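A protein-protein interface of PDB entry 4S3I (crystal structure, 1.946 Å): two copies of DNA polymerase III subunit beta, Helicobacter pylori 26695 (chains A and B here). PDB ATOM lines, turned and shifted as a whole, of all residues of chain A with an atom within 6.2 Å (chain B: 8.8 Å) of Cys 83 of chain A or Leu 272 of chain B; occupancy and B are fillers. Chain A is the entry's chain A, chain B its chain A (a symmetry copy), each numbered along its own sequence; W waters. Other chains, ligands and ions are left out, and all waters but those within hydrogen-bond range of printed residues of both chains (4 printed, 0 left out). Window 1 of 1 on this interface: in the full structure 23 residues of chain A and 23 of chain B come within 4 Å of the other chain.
Water W3 lies within hydrogen-bond range of the backbone carbonyl oxygen (O) of Cys 83 of chain A (2.6 Å) and the side-chain carboxylate (OE1) of Glu 268 of chain B (2.7 Å).
Water W2 bridges O of Ser 275 of chain B (2.6 Å) and OD2 of Asp 79 of chain A (2.7 Å).
Water W4 lies within hydrogen-bond range of the backbone carbonyl oxygen of Glu 268 of chain B (2.8 Å) and the backbone carbonyl oxygen of Cys 83 of chain A (2.9 Å).
Water W1 bridges O of Lys 271 of chain B (2.8 Å) and SG of Cys 83 of chain A (3.8 Å).
No position is printed for both chains.
Of the 10 pairs that touch across the chains among the printed residues, none has its exchanged pair printed and touching as well.
CG1 of Ile 80 of chain A touches OG of Ser 275 of chain B, 3.5 Å away.
CD1 of Leu 272 of chain B touches CB of Cys 83 of chain A, at 3.6 Å.
CD1 of Leu 272 of chain B touches CD2 of Leu 84 of chain A (3.8 Å).
Leu 272 of chain B touches Ser 105 of chain A.
Ser 105 of chain A touches Lys 303 of chain B (CA to O, 3.4 Å).
Leu 272 of chain B touches Phe 107 of chain A (CD1 to CZ, 3.3 Å).
Phe 107 of chain A touches Thr 301 of chain B.
CB of Ala 302 of chain B touches CD2 of Phe 107 of chain A, at 3.5 Å.
Of the printed residues of chain B, Cys 83 of chain A touches Leu 272.
Leu 272 of chain B touches just these residues of chain A: Cys 83, Leu 84, Ser 105 and Phe 107.
No residue of chain B comes within 4 Å of Ser 82 of chain A.
Of the printed residues of chain A, Lys 303 of chain B touches Ser 105.
Of the printed residues of chain A, Thr 301 of chain B touches Phe 107 (3.2 Å).
Of the printed residues of chain B, Phe 107 of chain A touches Leu 272 (3.3 Å), Thr 301 (3.2 Å) and Ala 302 (3.5 Å).
Of the printed residues of chain A, Thr 304 of chain B touches Ser 105 (2.7 Å).
Glu 13 of chain A touches none of the printed residues of chain B.
The nearest residue of chain A that does not touch Leu 272 of chain B is Ile 80 of chain A (4.1 Å).
The side-chain amino group of Lys 85 of chain A lies within salt-bridge range of the side-chain carboxylate of Glu 268 of chain B (3.1 Å).
OG1 of Thr 304 of chain B lies within hydrogen-bond range of OG of Ser 105 of chain A (2.7 Å).
Printed residues of chain B that touch a printed residue of chain A: Glu 268, Leu 272, Ser 275, Thr 301, Ala 302, Lys 303 and Thr 304.
Hydrophobic or aromatic side chains of chain B that line the printed part of chain A: Leu 272 and Ala 302.
Printed residues of chain A that touch a printed residue of chain B: Ile 80, Cys 83, Leu 84, Lys 85, Ser 105 and Phe 107.
Hydrophobic or aromatic side chains of chain A that line the printed part of chain B: Ile 80, Leu 84 and Phe 107.
Among the printed residues, 10 pairs touch across the chains.
Among the printed residues, Asp or Glu carboxylates within 4 Å of a Lys or Arg side-chain nitrogen of the other chain: Lys 85 of chain A with Glu 268 of chain B.
O of Asp 79 of chain A sits at hydrogen-bond distance from SG of Cys 83 of chain A.
OE1 of Gln 102 of chain A lies within hydrogen-bond range of N of Lys 85 of chain A (2.7 Å).
The backbone carbonyl oxygen of Leu 272 of chain B is in hydrogen-bond range of the side-chain hydroxyl of Ser 275 of chain B (2.9 Å).
The backbone carbonyl oxygen (O) of Thr 304 of chain B sits at hydrogen-bond distance from the backbone NH (N) of Phe 291 of chain B (2.7 Å).
The backbone carbonyl oxygen (O) of Ala 302 of chain B lies within hydrogen-bond range of the backbone NH (N) of Ser 293 of chain B, at 2.9 Å.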
ATOM      1  N   LYS A   9       5.654   1.959 -41.134  1.00  0.00           N
ATOM      2  CA  LYS A   9       5.640   2.259 -39.705  1.00  0.00           C
ATOM      3  C   LYS A   9       4.216   2.320 -39.156  1.00  0.00           C
ATOM      4  O   LYS A   9       3.901   1.719 -38.128  1.00  0.00           O
ATOM      5  CB  LYS A   9       6.383   3.583 -39.453  1.00  0.00           C
ATOM      6  CG  LYS A   9       6.625   3.941 -37.986  1.00  0.00           C
ATOM      7  CD  LYS A   9       5.433   4.656 -37.363  1.00  0.00           C
ATOM      8  CE  LYS A   9       5.874   5.707 -36.359  1.00  0.00           C
ATOM      9  NZ  LYS A   9       4.694   6.320 -35.683  1.00  0.00           N
ATOM     10  N   GLU A  13       2.595  -0.136 -36.472  1.00  0.00           N
ATOM     11  CA  GLU A  13       2.186   0.417 -35.179  1.00  0.00           C
ATOM     12  C   GLU A  13       0.722   0.100 -34.881  1.00  0.00           C
ATOM     13  O   GLU A  13       0.387  -0.375 -33.792  1.00  0.00           O
ATOM     14  CB  GLU A  13       2.431   1.929 -35.123  1.00  0.00           C
ATOM     15  CG  GLU A  13       1.950   2.594 -33.821  1.00  0.00           C
ATOM     16  CD  GLU A  13       2.398   4.052 -33.680  1.00  0.00           C
ATOM     17  OE1 GLU A  13       2.117   4.663 -32.629  1.00  0.00           O
ATOM     18  OE2 GLU A  13       3.028   4.588 -34.616  1.00  0.00           O
ATOM     19  N   LEU A  78       6.120  -2.442 -29.578  1.00  0.00           N
ATOM     20  CA  LEU A  78       5.289  -1.263 -29.799  1.00  0.00           C
ATOM     21  C   LEU A  78       5.946  -0.006 -29.223  1.00  0.00           C
ATOM     22  O   LEU A  78       5.872   1.077 -29.825  1.00  0.00           O
ATOM     23  CB  LEU A  78       3.900  -1.466 -29.207  1.00  0.00           C
ATOM     24  CG  LEU A  78       3.008  -0.225 -29.216  1.00  0.00           C
ATOM     25  CD1 LEU A  78       2.817   0.319 -30.632  1.00  0.00           C
ATOM     26  CD2 LEU A  78       1.668  -0.543 -28.573  1.00  0.00           C
ATOM     27  N   ASP A  79       6.594  -0.131 -28.070  1.00  0.00           N
ATOM     28  CA  ASP A  79       7.235   1.048 -27.476  1.00  0.00           C
ATOM     29  C   ASP A  79       8.285   1.620 -28.429  1.00  0.00           C
ATOM     30  O   ASP A  79       8.374   2.833 -28.604  1.00  0.00           O
ATOM     31  CB  ASP A  79       7.860   0.721 -26.107  1.00  0.00           C
ATOM     32  CG  ASP A  79       6.821   0.614 -24.994  1.00  0.00           C
ATOM     33  OD1 ASP A  79       5.718   1.165 -25.163  1.00  0.00           O
ATOM     34  OD2 ASP A  79       7.117  -0.022 -23.955  1.00  0.00           O
ATOM     35  N   ILE A  80       9.060   0.732 -29.054  1.00  0.00           N
ATOM     36  CA  ILE A  80      10.057   1.145 -30.039  1.00  0.00           C
ATOM     37  C   ILE A  80       9.421   1.783 -31.280  1.00  0.00           C
ATOM     38  O   ILE A  80       9.742   2.914 -31.632  1.00  0.00           O
ATOM     39  CB  ILE A  80      10.917  -0.044 -30.482  1.00  0.00           C
ATOM     40  CG1 ILE A  80      11.817  -0.518 -29.337  1.00  0.00           C
ATOM     41  CG2 ILE A  80      11.751   0.312 -31.707  1.00  0.00           C
ATOM     42  CD1 ILE A  80      12.567  -1.808 -29.667  1.00  0.00           C
ATOM     43  N   ILE A  81       8.518   1.057 -31.938  1.00  0.00           N
ATOM     44  CA  ILE A  81       7.880   1.553 -33.160  1.00  0.00           C
ATOM     45  C   ILE A  81       7.207   2.912 -32.963  1.00  0.00           C
ATOM     46  O   ILE A  81       7.335   3.807 -33.805  1.00  0.00           O
ATOM     47  CB  ILE A  81       6.854   0.541 -33.727  1.00  0.00           C
ATOM     48  CG1 ILE A  81       7.524  -0.796 -34.006  1.00  0.00           C
ATOM     49  CG2 ILE A  81       6.191   1.091 -34.994  1.00  0.00           C
ATOM     50  CD1 ILE A  81       8.809  -0.679 -34.821  1.00  0.00           C
ATOM     51  N   SER A  82       6.515   3.089 -31.840  1.00  0.00           N
ATOM     52  CA  SER A  82       5.768   4.328 -31.621  1.00  0.00           C
ATOM     53  C   SER A  82       6.699   5.539 -31.508  1.00  0.00           C
ATOM     54  O   SER A  82       6.277   6.686 -31.674  1.00  0.00           O
ATOM     55  CB  SER A  82       4.870   4.210 -30.385  1.00  0.00           C
ATOM     56  OG  SER A  82       5.634   4.043 -29.209  1.00  0.00           O
ATOM     57  N   CYS A  83       7.975   5.283 -31.241  1.00  0.00           N
ATOM     58  CA  CYS A  83       8.941   6.375 -31.100  1.00  0.00           C
ATOM     59  C   CYS A  83       9.736   6.645 -32.377  1.00  0.00           C
ATOM     60  O   CYS A  83      10.592   7.529 -32.400  1.00  0.00           O
ATOM     61  CB  CYS A  83       9.901   6.093 -29.932  1.00  0.00           C
ATOM     62  SG  CYS A  83       9.132   6.387 -28.329  1.00  0.00           S
ATOM     63  N   LEU A  84       9.450   5.892 -33.434  1.00  0.00           N
ATOM     64  CA  LEU A  84      10.223   6.003 -34.673  1.00  0.00           C
ATOM     65  C   LEU A  84       9.654   7.063 -35.615  1.00  0.00           C
ATOM     66  O   LEU A  84       8.633   7.688 -35.318  1.00  0.00           O
ATOM     67  CB  LEU A  84      10.311   4.648 -35.372  1.00  0.00           C
ATOM     68  CG  LEU A  84      11.290   3.690 -34.700  1.00  0.00           C
ATOM     69  CD1 LEU A  84      11.294   2.328 -35.379  1.00  0.00           C
ATOM     70  CD2 LEU A  84      12.688   4.298 -34.720  1.00  0.00           C
ATOM     71  N   LYS A  85      10.330   7.290 -36.737  1.00  0.00           N
ATOM     72  CA  LYS A  85       9.843   8.267 -37.709  1.00  0.00           C
ATOM     73  C   LYS A  85       8.755   7.626 -38.568  1.00  0.00           C
ATOM     74  O   LYS A  85       8.551   6.415 -38.516  1.00  0.00           O
ATOM     75  CB  LYS A  85      10.994   8.776 -38.589  1.00  0.00           C
ATOM     76  CG  LYS A  85      12.089   9.531 -37.830  1.00  0.00           C
ATOM     77  CD  LYS A  85      13.138  10.121 -38.775  1.00  0.00           C
ATOM     78  CE  LYS A  85      14.267  10.807 -38.007  1.00  0.00           C
ATOM     79  NZ  LYS A  85      13.743  11.823 -37.049  1.00  0.00           N
ATOM     80  N   GLN A 102      15.633   1.648 -38.833  1.00  0.00           N
ATOM     81  CA  GLN A 102      15.030   2.734 -39.579  1.00  0.00           C
ATOM     82  C   GLN A 102      16.104   3.798 -39.699  1.00  0.00           C
ATOM     83  O   GLN A 102      16.358   4.528 -38.740  1.00  0.00           O
ATOM     84  CB  GLN A 102      13.810   3.310 -38.854  1.00  0.00           C
ATOM     85  CG  GLN A 102      13.136   4.433 -39.625  1.00  0.00           C
ATOM     86  CD  GLN A 102      12.074   5.146 -38.821  1.00  0.00           C
ATOM     87  OE1 GLN A 102      12.382   5.908 -37.901  1.00  0.00           O
ATOM     88  NE2 GLN A 102      10.809   4.905 -39.162  1.00  0.00           N
ATOM     89  N   SER A 105      18.497   4.727 -36.844  1.00  0.00           N
ATOM     90  CA  SER A 105      18.078   4.032 -35.633  1.00  0.00           C
ATOM     91  C   SER A 105      18.110   2.528 -35.820  1.00  0.00           C
ATOM     92  O   SER A 105      17.735   2.013 -36.880  1.00  0.00           O
ATOM     93  CB  SER A 105      16.674   4.466 -35.226  1.00  0.00           C
ATOM     94  OG  SER A 105      16.615   5.864 -35.089  1.00  0.00           O
ATOM     95  N   PHE A 107      17.674  -1.405 -33.418  1.00  0.00           N
ATOM     96  CA  PHE A 107      17.383  -2.044 -32.146  1.00  0.00           C
ATOM     97  C   PHE A 107      17.524  -3.533 -32.272  1.00  0.00           C
ATOM     98  O   PHE A 107      17.403  -4.086 -33.369  1.00  0.00           O
ATOM     99  CB  PHE A 107      15.947  -1.759 -31.716  1.00  0.00           C
ATOM    100  CG  PHE A 107      15.559  -0.321 -31.806  1.00  0.00           C
ATOM    101  CD1 PHE A 107      15.250   0.255 -33.033  1.00  0.00           C
ATOM    102  CD2 PHE A 107      15.483   0.457 -30.663  1.00  0.00           C
ATOM    103  CE1 PHE A 107      14.897   1.579 -33.118  1.00  0.00           C
ATOM    104  CE2 PHE A 107      15.118   1.776 -30.739  1.00  0.00           C
ATOM    105  CZ  PHE A 107      14.826   2.340 -31.973  1.00  0.00           C
ATOM    106  N   GLU B 265      15.548  17.247 -31.526  1.00  0.00           N
ATOM    107  CA  GLU B 265      16.266  16.044 -31.954  1.00  0.00           C
ATOM    108  C   GLU B 265      16.761  15.230 -30.768  1.00  0.00           C
ATOM    109  O   GLU B 265      16.670  13.999 -30.762  1.00  0.00           O
ATOM    110  CB  GLU B 265      17.449  16.382 -32.862  1.00  0.00           C
ATOM    111  CG  GLU B 265      17.063  16.700 -34.294  1.00  0.00           C
ATOM    112  CD  GLU B 265      18.287  16.785 -35.203  1.00  0.00           C
ATOM    113  OE1 GLU B 265      19.332  17.309 -34.748  1.00  0.00           O
ATOM    114  OE2 GLU B 265      18.197  16.316 -36.361  1.00  0.00           O
ATOM    115  N   PHE B 266      17.307  15.910 -29.776  1.00  0.00           N
ATOM    116  CA  PHE B 266      17.722  15.213 -28.564  1.00  0.00           C
ATOM    117  C   PHE B 266      16.546  14.576 -27.799  1.00  0.00           C
ATOM    118  O   PHE B 266      16.671  13.445 -27.337  1.00  0.00           O
ATOM    119  CB  PHE B 266      18.574  16.126 -27.655  1.00  0.00           C
ATOM    120  CG  PHE B 266      20.049  16.026 -27.944  1.00  0.00           C
ATOM    121  CD1 PHE B 266      20.557  16.459 -29.168  1.00  0.00           C
ATOM    122  CD2 PHE B 266      20.906  15.440 -27.031  1.00  0.00           C
ATOM    123  CE1 PHE B 266      21.934  16.326 -29.464  1.00  0.00           C
ATOM    124  CE2 PHE B 266      22.272  15.311 -27.311  1.00  0.00           C
ATOM    125  CZ  PHE B 266      22.783  15.751 -28.535  1.00  0.00           C
ATOM    126  N   LYS B 267      15.432  15.300 -27.655  1.00  0.00           N
ATOM    127  CA  LYS B 267      14.246  14.736 -27.007  1.00  0.00           C
ATOM    128  C   LYS B 267      13.831  13.460 -27.732  1.00  0.00           C
ATOM    129  O   LYS B 267      13.583  12.439 -27.115  1.00  0.00           O
ATOM    130  CB  LYS B 267      13.061  15.717 -27.029  1.00  0.00           C
ATOM    131  CG  LYS B 267      13.098  16.868 -26.014  1.00  0.00           C
ATOM    132  CD  LYS B 267      11.821  17.722 -26.188  1.00  0.00           C
ATOM    133  CE  LYS B 267      11.772  18.899 -25.222  1.00  0.00           C
ATOM    134  NZ  LYS B 267      10.510  19.687 -25.412  1.00  0.00           N
ATOM    135  N   GLU B 268      13.768  13.539 -29.056  1.00  0.00           N
ATOM    136  CA  GLU B 268      13.269  12.434 -29.866  1.00  0.00           C
ATOM    137  C   GLU B 268      14.206  11.223 -29.748  1.00  0.00           C
ATOM    138  O   GLU B 268      13.764  10.078 -29.616  1.00  0.00           O
ATOM    139  CB  GLU B 268      13.127  12.903 -31.316  1.00  0.00           C
ATOM    140  CG  GLU B 268      12.436  11.944 -32.241  1.00  0.00           C
ATOM    141  CD  GLU B 268      12.433  12.447 -33.685  1.00  0.00           C
ATOM    142  OE1 GLU B 268      11.916  11.724 -34.568  1.00  0.00           O
ATOM    143  OE2 GLU B 268      12.954  13.563 -33.932  1.00  0.00           O
ATOM    144  N   SER B 269      15.506  11.488 -29.745  1.00  0.00           N
ATOM    145  CA  SER B 269      16.506  10.427 -29.696  1.00  0.00           C
ATOM    146  C   SER B 269      16.540   9.755 -28.324  1.00  0.00           C
ATOM    147  O   SER B 269      16.649   8.529 -28.226  1.00  0.00           O
ATOM    148  CB  SER B 269      17.883  10.992 -30.065  1.00  0.00           C
ATOM    149  OG  SER B 269      17.893  11.419 -31.418  1.00  0.00           O
ATOM    150  N   ILE B 270      16.441  10.568 -27.277  1.00  0.00           N
ATOM    151  CA  ILE B 270      16.433  10.071 -25.903  1.00  0.00           C
ATOM    152  C   ILE B 270      15.185   9.238 -25.590  1.00  0.00           C
ATOM    153  O   ILE B 270      15.282   8.164 -24.979  1.00  0.00           O
ATOM    154  CB  ILE B 270      16.582  11.233 -24.915  1.00  0.00           C
ATOM    155  CG1 ILE B 270      18.010  11.776 -25.012  1.00  0.00           C
ATOM    156  CG2 ILE B 270      16.272  10.783 -23.489  1.00  0.00           C
ATOM    157  CD1 ILE B 270      18.177  13.151 -24.424  1.00  0.00           C
ATOM    158  N   LYS B 271      14.018   9.719 -26.011  1.00  0.00           N
ATOM    159  CA  LYS B 271      12.793   8.932 -25.863  1.00  0.00           C
ATOM    160  C   LYS B 271      12.933   7.594 -26.562  1.00  0.00           C
ATOM    161  O   LYS B 271      12.510   6.555 -26.049  1.00  0.00           O
ATOM    162  CB  LYS B 271      11.587   9.685 -26.428  1.00  0.00           C
ATOM    163  CG  LYS B 271      11.187  10.892 -25.610  1.00  0.00           C
ATOM    164  CD  LYS B 271      10.077  11.685 -26.292  1.00  0.00           C
ATOM    165  CE  LYS B 271       9.674  12.886 -25.438  1.00  0.00           C
ATOM    166  NZ  LYS B 271       8.809  13.867 -26.172  1.00  0.00           N
ATOM    167  N   LEU B 272      13.531   7.630 -27.746  1.00  0.00           N
ATOM    168  CA  LEU B 272      13.709   6.437 -28.563  1.00  0.00           C
ATOM    169  C   LEU B 272      14.508   5.361 -27.819  1.00  0.00           C
ATOM    170  O   LEU B 272      14.123   4.193 -27.808  1.00  0.00           O
ATOM    171  CB  LEU B 272      14.421   6.817 -29.866  1.00  0.00           C
ATOM    172  CG  LEU B 272      14.547   5.726 -30.915  1.00  0.00           C
ATOM    173  CD1 LEU B 272      13.204   5.033 -31.022  1.00  0.00           C
ATOM    174  CD2 LEU B 272      14.944   6.296 -32.272  1.00  0.00           C
ATOM    175  N   CYS B 273      15.621   5.745 -27.199  1.00  0.00           N
ATOM    176  CA  CYS B 273      16.439   4.762 -26.474  1.00  0.00           C
ATOM    177  C   CYS B 273      15.785   4.397 -25.147  1.00  0.00           C
ATOM    178  O   CYS B 273      15.999   3.307 -24.619  1.00  0.00           O
ATOM    179  CB  CYS B 273      17.869   5.282 -26.261  1.00  0.00           C
ATOM    180  SG  CYS B 273      18.801   5.481 -27.805  1.00  0.00           S
ATOM    181  N   SER B 274      14.960   5.311 -24.640  1.00  0.00           N
ATOM    182  CA  SER B 274      14.254   5.125 -23.369  1.00  0.00           C
ATOM    183  C   SER B 274      13.233   4.014 -23.432  1.00  0.00           C
ATOM    184  O   SER B 274      12.686   3.609 -22.409  1.00  0.00           O
ATOM    185  CB  SER B 274      13.528   6.407 -22.957  1.00  0.00           C
ATOM    186  OG  SER B 274      14.445   7.354 -22.476  1.00  0.00           O
ATOM    187  N   SER B 275      12.948   3.542 -24.637  1.00  0.00           N
ATOM    188  CA  SER B 275      12.006   2.456 -24.797  1.00  0.00           C
ATOM    189  C   SER B 275      12.565   1.201 -24.139  1.00  0.00           C
ATOM    190  O   SER B 275      11.808   0.333 -23.695  1.00  0.00           O
ATOM    191  CB  SER B 275      11.732   2.199 -26.271  1.00  0.00           C
ATOM    192  OG  SER B 275      12.897   1.749 -26.924  1.00  0.00           O
ATOM    193  N   LEU B 276      13.892   1.116 -24.060  1.00  0.00           N
ATOM    194  CA  LEU B 276      14.544  -0.094 -23.558  1.00  0.00           C
ATOM    195  C   LEU B 276      15.439   0.120 -22.324  1.00  0.00           C
ATOM    196  O   LEU B 276      16.004  -0.839 -21.799  1.00  0.00           O
ATOM    197  CB  LEU B 276      15.355  -0.767 -24.674  1.00  0.00           C
ATOM    198  CG  LEU B 276      14.572  -1.400 -25.823  1.00  0.00           C
ATOM    199  CD1 LEU B 276      15.509  -2.179 -26.746  1.00  0.00           C
ATOM    200  CD2 LEU B 276      13.484  -2.321 -25.263  1.00  0.00           C
ATOM    201  N   SER B 277      15.574   1.360 -21.868  1.00  0.00           N
ATOM    202  CA  SER B 277      16.495   1.657 -20.763  1.00  0.00           C
ATOM    203  C   SER B 277      16.099   2.929 -20.020  1.00  0.00           C
ATOM    204  O   SER B 277      15.299   3.715 -20.521  1.00  0.00           O
ATOM    205  CB  SER B 277      17.911   1.827 -21.303  1.00  0.00           C
ATOM    206  OG  SER B 277      17.984   2.985 -22.112  1.00  0.00           O
ATOM    207  N   ILE B 280      21.252   6.266 -20.587  1.00  0.00           N
ATOM    208  CA  ILE B 280      21.674   6.342 -21.973  1.00  0.00           C
ATOM    209  C   ILE B 280      23.134   6.769 -22.056  1.00  0.00           C
ATOM    210  O   ILE B 280      23.569   7.664 -21.328  1.00  0.00           O
ATOM    211  CB  ILE B 280      20.790   7.369 -22.728  1.00  0.00           C
ATOM    212  CG1 ILE B 280      19.409   6.771 -23.022  1.00  0.00           C
ATOM    213  CG2 ILE B 280      21.445   7.829 -24.028  1.00  0.00           C
ATOM    214  CD1 ILE B 280      18.413   7.800 -23.547  1.00  0.00           C
ATOM    215  N   PHE B 291      23.421   7.928 -29.626  1.00  0.00           N
ATOM    216  CA  PHE B 291      22.698   7.586 -28.405  1.00  0.00           C
ATOM    217  C   PHE B 291      22.570   6.075 -28.304  1.00  0.00           C
ATOM    218  O   PHE B 291      22.117   5.435 -29.246  1.00  0.00           O
ATOM    219  CB  PHE B 291      21.292   8.197 -28.421  1.00  0.00           C
ATOM    220  CG  PHE B 291      21.258   9.691 -28.650  1.00  0.00           C
ATOM    221  CD1 PHE B 291      20.981  10.563 -27.600  1.00  0.00           C
ATOM    222  CD2 PHE B 291      21.456  10.220 -29.923  1.00  0.00           C
ATOM    223  CE1 PHE B 291      20.925  11.946 -27.807  1.00  0.00           C
ATOM    224  CE2 PHE B 291      21.403  11.597 -30.147  1.00  0.00           C
ATOM    225  CZ  PHE B 291      21.132  12.465 -29.091  1.00  0.00           C
ATOM    226  N   GLU B 292      22.956   5.505 -27.160  1.00  0.00           N
ATOM    227  CA  GLU B 292      22.859   4.059 -26.950  1.00  0.00           C
ATOM    228  C   GLU B 292      22.242   3.746 -25.598  1.00  0.00           C
ATOM    229  O   GLU B 292      22.595   4.364 -24.596  1.00  0.00           O
ATOM    230  CB  GLU B 292      24.248   3.397 -27.013  1.00  0.00           C
ATOM    231  CG  GLU B 292      24.890   3.368 -28.395  1.00  0.00           C
ATOM    232  CD  GLU B 292      26.334   2.878 -28.382  1.00  0.00           C
ATOM    233  OE1 GLU B 292      27.203   3.594 -27.835  1.00  0.00           O
ATOM    234  OE2 GLU B 292      26.596   1.781 -28.925  1.00  0.00           O
ATOM    235  N   SER B 293      21.345   2.769 -25.568  1.00  0.00           N
ATOM    236  CA  SER B 293      20.749   2.328 -24.309  1.00  0.00           C
ATOM    237  C   SER B 293      21.852   1.790 -23.407  1.00  0.00           C
ATOM    238  O   SER B 293      22.771   1.125 -23.882  1.00  0.00           O
ATOM    239  CB  SER B 293      19.697   1.250 -24.555  1.00  0.00           C
ATOM    240  OG  SER B 293      20.255   0.120 -25.199  1.00  0.00           O
ATOM    241  N   THR B 301      18.912  -3.974 -27.062  1.00  0.00           N
ATOM    242  CA  THR B 301      19.697  -2.764 -27.344  1.00  0.00           C
ATOM    243  C   THR B 301      18.929  -1.766 -28.215  1.00  0.00           C
ATOM    244  O   THR B 301      18.101  -2.160 -29.040  1.00  0.00           O
ATOM    245  CB  THR B 301      21.064  -3.059 -28.024  1.00  0.00           C
ATOM    246  OG1 THR B 301      20.867  -3.288 -29.423  1.00  0.00           O
ATOM    247  CG2 THR B 301      21.751  -4.264 -27.400  1.00  0.00           C
ATOM    248  N   ALA B 302      19.224  -0.482 -28.021  1.00  0.00           N
ATOM    249  CA  ALA B 302      18.631   0.604 -28.790  1.00  0.00           C
ATOM    250  C   ALA B 302      19.758   1.559 -29.126  1.00  0.00           C
ATOM    251  O   ALA B 302      20.514   1.953 -28.241  1.00  0.00           O
ATOM    252  CB  ALA B 302      17.552   1.327 -27.973  1.00  0.00           C
ATOM    253  N   LYS B 303      19.893   1.918 -30.399  1.00  0.00           N
ATOM    254  CA  LYS B 303      20.873   2.920 -30.801  1.00  0.00           C
ATOM    255  C   LYS B 303      20.234   3.876 -31.785  1.00  0.00           C
ATOM    256  O   LYS B 303      19.366   3.479 -32.578  1.00  0.00           O
ATOM    257  CB  LYS B 303      22.098   2.286 -31.488  1.00  0.00           C
ATOM    258  CG  LYS B 303      22.410   0.837 -31.126  1.00  0.00           C
ATOM    259  CD  LYS B 303      23.819   0.437 -31.586  1.00  0.00           C
ATOM    260  CE  LYS B 303      24.136   0.984 -32.974  1.00  0.00           C
ATOM    261  NZ  LYS B 303      25.471   0.543 -33.485  1.00  0.00           N
ATOM    262  N   THR B 304      20.686   5.123 -31.765  1.00  0.00           N
ATOM    263  CA  THR B 304      20.351   6.051 -32.839  1.00  0.00           C
ATOM    264  C   THR B 304      21.383   7.154 -32.879  1.00  0.00           C
ATOM    265  O   THR B 304      22.171   7.316 -31.944  1.00  0.00           O
ATOM    266  CB  THR B 304      18.946   6.670 -32.675  1.00  0.00           C
ATOM    267  OG1 THR B 304      18.559   7.303 -33.904  1.00  0.00           O
ATOM    268  CG2 THR B 304      18.945   7.698 -31.570  1.00  0.00           C
ATOM    269  N   SER B 305      21.393   7.908 -33.970  1.00  0.00           N
ATOM    270  CA  SER B 305      22.288   9.039 -34.062  1.00  0.00           C
ATOM    271  C   SER B 305      21.645  10.177 -34.830  1.00  0.00           C
ATOM    272  O   SER B 305      20.660  10.004 -35.555  1.00  0.00           O
ATOM    273  CB  SER B 305      23.631   8.649 -34.691  1.00  0.00           C
ATOM    274  OG  SER B 305      23.479   8.277 -36.048  1.00  0.00           O
ATOM    275  N   VAL B 306      22.236  11.345 -34.655  1.00  0.00           N
ATOM    276  CA  VAL B 306      21.766  12.556 -35.273  1.00  0.00           C
ATOM    277  C   VAL B 306      22.988  13.295 -35.847  1.00  0.00           C
ATOM    278  O   VAL B 306      24.025  13.405 -35.189  1.00  0.00           O
ATOM    279  CB  VAL B 306      21.012  13.386 -34.213  1.00  0.00           C
ATOM    280  CG1 VAL B 306      21.327  14.866 -34.332  1.00  0.00           C
ATOM    281  CG2 VAL B 306      19.516  13.106 -34.292  1.00  0.00           C
ATOM    282  N   ALA B 324      17.909   9.303 -18.539  1.00  0.00           N
ATOM    283  CA  ALA B 324      17.085   9.709 -19.675  1.00  0.00           C
ATOM    284  C   ALA B 324      15.972  10.658 -19.239  1.00  0.00           C
ATOM    285  O   ALA B 324      15.788  11.741 -19.814  1.00  0.00           O
ATOM    286  CB  ALA B 324      16.512   8.472 -20.375  1.00  0.00           C
ATOM    287  N   LEU B 328      15.515  14.535 -20.301  1.00  0.00           N
ATOM    288  CA  LEU B 328      14.302  14.964 -20.992  1.00  0.00           C
ATOM    289  C   LEU B 328      13.620  16.090 -20.232  1.00  0.00           C
ATOM    290  O   LEU B 328      13.185  17.082 -20.824  1.00  0.00           O
ATOM    291  CB  LEU B 328      13.323  13.797 -21.174  1.00  0.00           C
ATOM    292  CG  LEU B 328      13.654  12.825 -22.285  1.00  0.00           C
ATOM    293  CD1 LEU B 328      12.676  11.644 -22.283  1.00  0.00           C
ATOM    294  CD2 LEU B 328      13.631  13.548 -23.629  1.00  0.00           C
HETATM  295  O   HOH W   1      10.107   6.006 -24.722  1.00  0.00           O
HETATM  296  O   HOH W   2       9.578  -1.063 -23.566  1.00  0.00           O
HETATM  297  O   HOH W   3      11.996   9.117 -33.943  1.00  0.00           O
HETATM  298  O   HOH W   4      11.154   9.477 -30.290  1.00  0.00           O
